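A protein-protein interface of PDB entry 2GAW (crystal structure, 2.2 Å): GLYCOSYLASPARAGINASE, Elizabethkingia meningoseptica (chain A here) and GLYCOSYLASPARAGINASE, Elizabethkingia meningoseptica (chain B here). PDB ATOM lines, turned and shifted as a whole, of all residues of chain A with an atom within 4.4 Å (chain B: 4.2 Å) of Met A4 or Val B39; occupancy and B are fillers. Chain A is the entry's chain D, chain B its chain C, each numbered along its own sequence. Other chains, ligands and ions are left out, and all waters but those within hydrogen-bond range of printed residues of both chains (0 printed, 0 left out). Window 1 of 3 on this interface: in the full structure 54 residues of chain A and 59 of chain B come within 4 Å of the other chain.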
ATOM      1  N   ILE A   2      15.926  22.435 -28.896  1.00  0.00           N
ATOM      2  CA  ILE A   2      14.774  22.639 -28.054  1.00  0.00           C
ATOM      3  C   ILE A   2      15.307  23.503 -26.909  1.00  0.00           C
ATOM      4  O   ILE A   2      16.427  23.326 -26.409  1.00  0.00           O
ATOM      5  CB  ILE A   2      14.197  21.269 -27.579  1.00  0.00           C
ATOM      6  CG1 ILE A   2      12.878  21.595 -26.873  1.00  0.00           C
ATOM      7  CG2 ILE A   2      15.171  20.478 -26.718  1.00  0.00           C
ATOM      8  CD1 ILE A   2      12.006  20.385 -26.518  1.00  0.00           C
ATOM      9  N   GLY A   3      14.559  24.555 -26.641  1.00  0.00           N
ATOM     10  CA  GLY A   3      14.822  25.405 -25.516  1.00  0.00           C
ATOM     11  C   GLY A   3      13.619  25.253 -24.606  1.00  0.00           C
ATOM     12  O   GLY A   3      12.498  25.153 -25.129  1.00  0.00           O
ATOM     13  N   MET A   4      13.802  25.228 -23.282  1.00  0.00           N
ATOM     14  CA  MET A   4      12.719  25.062 -22.341  1.00  0.00           C
ATOM     15  C   MET A   4      12.950  25.909 -21.118  1.00  0.00           C
ATOM     16  O   MET A   4      14.034  25.843 -20.533  1.00  0.00           O
ATOM     17  CB  MET A   4      12.608  23.621 -21.885  1.00  0.00           C
ATOM     18  CG  MET A   4      11.369  23.373 -21.042  1.00  0.00           C
ATOM     19  SD  MET A   4      11.285  21.645 -20.521  1.00  0.00           S
ATOM     20  CE  MET A   4      10.259  21.056 -21.830  1.00  0.00           C
ATOM     21  N   ILE A   5      11.951  26.670 -20.695  1.00  0.00           N
ATOM     22  CA  ILE A   5      12.045  27.478 -19.487  1.00  0.00           C
ATOM     23  C   ILE A   5      10.839  27.158 -18.594  1.00  0.00           C
ATOM     24  O   ILE A   5       9.775  26.769 -19.115  1.00  0.00           O
ATOM     25  CB  ILE A   5      12.075  28.999 -19.847  1.00  0.00           C
ATOM     26  CG1 ILE A   5      10.934  29.385 -20.799  1.00  0.00           C
ATOM     27  CG2 ILE A   5      13.469  29.315 -20.412  1.00  0.00           C
ATOM     28  CD1 ILE A   5      10.822  30.894 -21.081  1.00  0.00           C
ATOM     29  N   SER A  14      14.004  28.355 -14.099  1.00  0.00           N
ATOM     30  CA  SER A  14      15.166  27.635 -14.591  1.00  0.00           C
ATOM     31  C   SER A  14      14.896  27.341 -16.057  1.00  0.00           C
ATOM     32  O   SER A  14      13.746  27.430 -16.511  1.00  0.00           O
ATOM     33  CB  SER A  14      15.380  26.314 -13.869  1.00  0.00           C
ATOM     34  OG  SER A  14      15.891  26.454 -12.545  1.00  0.00           O
ATOM     35  N   GLY A  15      15.940  27.022 -16.812  1.00  0.00           N
ATOM     36  CA  GLY A  15      15.788  26.733 -18.220  1.00  0.00           C
ATOM     37  C   GLY A  15      16.903  25.849 -18.729  1.00  0.00           C
ATOM     38  O   GLY A  15      17.942  25.710 -18.073  1.00  0.00           O
ATOM     39  N   ALA A  16      16.696  25.284 -19.914  1.00  0.00           N
ATOM     40  CA  ALA A  16      17.612  24.344 -20.536  1.00  0.00           C
ATOM     41  C   ALA A  16      17.558  24.555 -22.043  1.00  0.00           C
ATOM     42  O   ALA A  16      16.533  24.998 -22.570  1.00  0.00           O
ATOM     43  CB  ALA A  16      17.194  22.911 -20.232  1.00  0.00           C
ATOM     44  N   THR A  18      19.194  22.747 -25.798  1.00  0.00           N
ATOM     45  CA  THR A  18      19.948  21.639 -26.356  1.00  0.00           C
ATOM     46  C   THR A  18      19.753  21.531 -27.862  1.00  0.00           C
ATOM     47  O   THR A  18      18.636  21.702 -28.374  1.00  0.00           O
ATOM     48  CB  THR A  18      19.514  20.278 -25.805  1.00  0.00           C
ATOM     49  OG1 THR A  18      18.903  20.378 -24.522  1.00  0.00           O
ATOM     50  CG2 THR A  18      20.747  19.432 -25.813  1.00  0.00           C
ATOM     51  N   THR A  50      14.178  31.866 -23.962  1.00  0.00           N
ATOM     52  CA  THR A  50      15.001  30.992 -24.792  1.00  0.00           C
ATOM     53  C   THR A  50      14.798  31.440 -26.235  1.00  0.00           C
ATOM     54  O   THR A  50      13.698  31.895 -26.588  1.00  0.00           O
ATOM     55  CB  THR A  50      14.619  29.482 -24.800  1.00  0.00           C
ATOM     56  OG1 THR A  50      13.492  29.245 -23.974  1.00  0.00           O
ATOM     57  CG2 THR A  50      15.806  28.669 -24.378  1.00  0.00           C
ATOM     58  N   VAL B   7       5.447  25.714 -17.930  1.00  0.00           N
ATOM     59  CA  VAL B   7       6.603  25.381 -18.753  1.00  0.00           C
ATOM     60  C   VAL B   7       6.338  25.883 -20.169  1.00  0.00           C
ATOM     61  O   VAL B   7       5.202  25.742 -20.653  1.00  0.00           O
ATOM     62  CB  VAL B   7       6.897  23.873 -19.027  1.00  0.00           C
ATOM     63  CG1 VAL B   7       8.363  23.644 -18.763  1.00  0.00           C
ATOM     64  CG2 VAL B   7       5.974  22.957 -18.273  1.00  0.00           C
ATOM     65  N   LEU B   8       7.352  26.428 -20.847  1.00  0.00           N
ATOM     66  CA  LEU B   8       7.257  26.757 -22.258  1.00  0.00           C
ATOM     67  C   LEU B   8       8.457  26.113 -22.939  1.00  0.00           C
ATOM     68  O   LEU B   8       9.572  26.148 -22.399  1.00  0.00           O
ATOM     69  CB  LEU B   8       7.390  28.234 -22.613  1.00  0.00           C
ATOM     70  CG  LEU B   8       6.771  29.407 -21.891  1.00  0.00           C
ATOM     71  CD1 LEU B   8       6.842  30.580 -22.849  1.00  0.00           C
ATOM     72  CD2 LEU B   8       5.328  29.193 -21.528  1.00  0.00           C
ATOM     73  N   SER B   9       8.268  25.528 -24.114  1.00  0.00           N
ATOM     74  CA  SER B   9       9.375  25.035 -24.905  1.00  0.00           C
ATOM     75  C   SER B   9       9.175  25.377 -26.383  1.00  0.00           C
ATOM     76  O   SER B   9       8.076  25.743 -26.829  1.00  0.00           O
ATOM     77  CB  SER B   9       9.503  23.533 -24.717  1.00  0.00           C
ATOM     78  OG  SER B   9       8.250  22.891 -24.810  1.00  0.00           O
ATOM     79  N   ALA B  17       7.652  17.246 -24.907  1.00  0.00           N
ATOM     80  CA  ALA B  17       8.665  17.591 -23.904  1.00  0.00           C
ATOM     81  C   ALA B  17       8.034  18.173 -22.642  1.00  0.00           C
ATOM     82  O   ALA B  17       8.383  17.822 -21.503  1.00  0.00           O
ATOM     83  CB  ALA B  17       9.627  18.619 -24.470  1.00  0.00           C
ATOM     84  N   ASN B  18       7.021  19.005 -22.864  1.00  0.00           N
ATOM     85  CA  ASN B  18       6.275  19.654 -21.806  1.00  0.00           C
ATOM     86  C   ASN B  18       5.567  18.669 -20.893  1.00  0.00           C
ATOM     87  O   ASN B  18       5.417  18.927 -19.700  1.00  0.00           O
ATOM     88  CB  ASN B  18       5.247  20.604 -22.398  1.00  0.00           C
ATOM     89  CG  ASN B  18       5.743  22.030 -22.556  1.00  0.00           C
ATOM     90  OD1 ASN B  18       6.923  22.355 -22.411  1.00  0.00           O
ATOM     91  ND2 ASN B  18       4.835  22.945 -22.833  1.00  0.00           N
ATOM     92  N   ALA B  21       8.328  17.362 -18.450  1.00  0.00           N
ATOM     93  CA  ALA B  21       8.611  18.433 -17.510  1.00  0.00           C
ATOM     94  C   ALA B  21       7.474  18.590 -16.500  1.00  0.00           C
ATOM     95  O   ALA B  21       7.701  18.761 -15.296  1.00  0.00           O
ATOM     96  CB  ALA B  21       8.784  19.749 -18.260  1.00  0.00           C
ATOM     97  N   VAL B  35      12.921  21.095 -16.389  1.00  0.00           N
ATOM     98  CA  VAL B  35      13.432  21.474 -17.705  1.00  0.00           C
ATOM     99  C   VAL B  35      14.483  20.488 -18.173  1.00  0.00           C
ATOM    100  O   VAL B  35      14.542  20.235 -19.377  1.00  0.00           O
ATOM    101  CB  VAL B  35      14.038  22.928 -17.707  1.00  0.00           C
ATOM    102  CG1 VAL B  35      12.898  23.873 -17.367  1.00  0.00           C
ATOM    103  CG2 VAL B  35      15.204  23.115 -16.717  1.00  0.00           C
ATOM    104  N   GLU B  36      15.282  19.889 -17.276  1.00  0.00           N
ATOM    105  CA  GLU B  36      16.255  18.876 -17.664  1.00  0.00           C
ATOM    106  C   GLU B  36      15.551  17.615 -18.164  1.00  0.00           C
ATOM    107  O   GLU B  36      15.851  17.116 -19.256  1.00  0.00           O
ATOM    108  CB  GLU B  36      17.142  18.503 -16.490  1.00  0.00           C
ATOM    109  CG  GLU B  36      18.270  17.569 -16.936  1.00  0.00           C
ATOM    110  CD  GLU B  36      19.056  16.873 -15.839  1.00  0.00           C
ATOM    111  OE1 GLU B  36      18.627  16.830 -14.686  1.00  0.00           O
ATOM    112  OE2 GLU B  36      20.126  16.353 -16.132  1.00  0.00           O
ATOM    113  N   LYS B  37      14.568  17.110 -17.401  1.00  0.00           N
ATOM    114  CA  LYS B  37      13.786  15.946 -17.813  1.00  0.00           C
ATOM    115  C   LYS B  37      13.072  16.191 -19.137  1.00  0.00           C
ATOM    116  O   LYS B  37      13.062  15.315 -20.008  1.00  0.00           O
ATOM    117  CB  LYS B  37      12.685  15.573 -16.828  1.00  0.00           C
ATOM    118  CG  LYS B  37      13.056  15.135 -15.422  1.00  0.00           C
ATOM    119  CD  LYS B  37      13.918  13.880 -15.349  1.00  0.00           C
ATOM    120  CE  LYS B  37      13.800  13.248 -13.951  1.00  0.00           C
ATOM    121  NZ  LYS B  37      14.189  14.165 -12.889  1.00  0.00           N
ATOM    122  N   GLY B  38      12.498  17.383 -19.290  1.00  0.00           N
ATOM    123  CA  GLY B  38      11.788  17.769 -20.487  1.00  0.00           C
ATOM    124  C   GLY B  38      12.618  17.671 -21.756  1.00  0.00           C
ATOM    125  O   GLY B  38      12.228  16.994 -22.714  1.00  0.00           O
ATOM    126  N   VAL B  39      13.788  18.315 -21.808  1.00  0.00           N
ATOM    127  CA  VAL B  39      14.582  18.300 -23.036  1.00  0.00           C
ATOM    128  C   VAL B  39      15.269  16.968 -23.322  1.00  0.00           C
ATOM    129  O   VAL B  39      15.378  16.572 -24.489  1.00  0.00           O
ATOM    130  CB  VAL B  39      15.612  19.454 -22.998  1.00  0.00           C
ATOM    131  CG1 VAL B  39      14.792  20.743 -22.884  1.00  0.00           C
ATOM    132  CG2 VAL B  39      16.616  19.332 -21.862  1.00  0.00           C
ATOM    133  N   ARG B  40      15.621  16.219 -22.275  1.00  0.00           N
ATOM    134  CA  ARG B  40      16.208  14.891 -22.411  1.00  0.00           C
ATOM    135  C   ARG B  40      15.385  13.977 -23.284  1.00  0.00           C
ATOM    136  O   ARG B  40      15.932  13.256 -24.097  1.00  0.00           O
ATOM    137  CB  ARG B  40      16.332  14.217 -21.097  1.00  0.00           C
ATOM    138  CG  ARG B  40      17.561  14.628 -20.343  1.00  0.00           C
ATOM    139  CD  ARG B  40      17.423  13.914 -19.027  1.00  0.00           C
ATOM    140  NE  ARG B  40      18.741  13.463 -18.678  1.00  0.00           N
ATOM    141  CZ  ARG B  40      19.199  12.255 -18.978  1.00  0.00           C
ATOM    142  NH1 ARG B  40      18.444  11.354 -19.613  1.00  0.00           N
ATOM    143  NH2 ARG B  40      20.478  12.044 -18.689  1.00  0.00           N
ATOM    144  N   LEU B  41      14.053  14.075 -23.203  1.00  0.00           N
ATOM    145  CA  LEU B  41      13.141  13.302 -24.035  1.00  0.00           C
ATOM    146  C   LEU B  41      13.490  13.465 -25.512  1.00  0.00           C
ATOM    147  O   LEU B  41      13.668  12.503 -26.250  1.00  0.00           O
ATOM    148  CB  LEU B  41      11.723  13.791 -23.774  1.00  0.00           C
ATOM    149  CG  LEU B  41      10.579  13.084 -24.480  1.00  0.00           C
ATOM    150  CD1 LEU B  41      10.269  11.747 -23.810  1.00  0.00           C
ATOM    151  CD2 LEU B  41       9.370  13.971 -24.424  1.00  0.00           C
ATOM    152  N   VAL B  42      13.702  14.711 -25.918  1.00  0.00           N
ATOM    153  CA  VAL B  42      13.995  15.053 -27.298  1.00  0.00           C
ATOM    154  C   VAL B  42      15.416  14.617 -27.632  1.00  0.00           C
ATOM    155  O   VAL B  42      15.621  14.065 -28.701  1.00  0.00           O
ATOM    156  CB  VAL B  42      13.759  16.586 -27.453  1.00  0.00           C
ATOM    157  CG1 VAL B  42      13.844  17.033 -28.914  1.00  0.00           C
ATOM    158  CG2 VAL B  42      12.345  16.910 -26.962  1.00  0.00           C
ATOM    159  N   GLU B  43      16.419  14.765 -26.760  1.00  0.00           N
ATOM    160  CA  GLU B  43      17.774  14.282 -27.026  1.00  0.00           C
ATOM    161  C   GLU B  43      17.799  12.762 -27.222  1.00  0.00           C
ATOM    162  O   GLU B  43      18.618  12.195 -27.962  1.00  0.00           O
ATOM    163  CB  GLU B  43      18.728  14.574 -25.871  1.00  0.00           C
ATOM    164  CG  GLU B  43      18.912  16.018 -25.408  1.00  0.00           C
ATOM    165  CD  GLU B  43      19.797  16.171 -24.172  1.00  0.00           C
ATOM    166  OE1 GLU B  43      19.762  15.366 -23.252  1.00  0.00           O
ATOM    167  OE2 GLU B  43      20.547  17.134 -24.081  1.00  0.00           O
ATOM    168  N   ILE B  89      22.586  17.984 -22.060  1.00  0.00           N
ATOM    169  CA  ILE B  89      22.042  18.816 -21.004  1.00  0.00           C
ATOM    170  C   ILE B  89      22.469  18.320 -19.615  1.00  0.00           C
ATOM    171  O   ILE B  89      22.793  19.142 -18.746  1.00  0.00           O
ATOM    172  CB  ILE B  89      20.485  18.872 -21.162  1.00  0.00           C
ATOM    173  CG1 ILE B  89      19.958  20.048 -20.362  1.00  0.00           C
ATOM    174  CG2 ILE B  89      19.814  17.589 -20.685  1.00  0.00           C
ATOM    175  CD1 ILE B  89      20.452  21.440 -20.815  1.00  0.00           C
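The side-chain amide oxygen (OD1) of Asn B18 lies within hydrogen-bond range of the side-chain hydroxyl (OG) of Ser B9 (2.8 Å). The side-chain carboxylate of Glu B43 is in hydrogen-bond range of the backbone NH of Ile B89 (3.0 Å). The backbone NH of Ile A2 lies within hydrogen-bond range of the backbone carbonyl oxygen of Thr A18 (2.9 Å). N of Ala A16 sits at hydrogen-bond distance from O of Met A4 (2.8 Å).
O of Leu B8 sits at hydrogen-bond distance from N of Ile A5 (3.0 Å). SD of Met A4 sits close to O of Val B35, 3.7 Å away.
Printed residues of chain B within 4 Å of Gly A3: Ser B9. Met A4 touches nine residues of chain B. Of the printed residues of chain A, Val B7 touches Met A4 (3.8 Å) and Ile A5 (3.4 Å). Val B39 touches just these residues of chain A: Ile A2, Met A4, Ala A16 and Thr A18. The nearest printed residue of chain B that does not touch Met A4 is Glu B36 (5.4 Å). The nearest printed residue of chain A that does not touch Val B39 is Gly A3 (5.0 Å).
Hydrophobic or aromatic side chains of chain A within 4 Å of the printed part of chain B: Ile A2, Met A4, Ile A5 and Ala A16. Of the 16 printed residues of chain B, 12 touch a printed residue of chain A. Hydrophobic or aromatic side chains of chain B that line the printed part of chain A: Val B7, Ala B17, Ala B21, Val B35, Val B39, Val B42 and Ile B89. Among the printed residues, 22 pairs touch across the chains. Among the printed residues, no Asp or Glu carboxylate lies within 4 Å of a Lys or Arg side-chain nitrogen of the other chain.
Ile A2 touches Ala B17. CG2 of Ile A2 touches CG1 of Val B39, at 3.9 Å. CA of Met A4 touches O of Leu B8, 3.3 Å away. CB of Met A4 touches CG1 of Val B39, 3.7 Å away. O of Ile A5 touches CG1 of Val B7, at 3.4 Å. Val B35 touches Ser A14. C of Gly A15 touches CG2 of Val B35 (3.8 Å). Ala A16 touches Val B35. Ala A16 touches Val B39 (CB to CG2, 3.97 Å). Ala A16 touches Ile B89.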
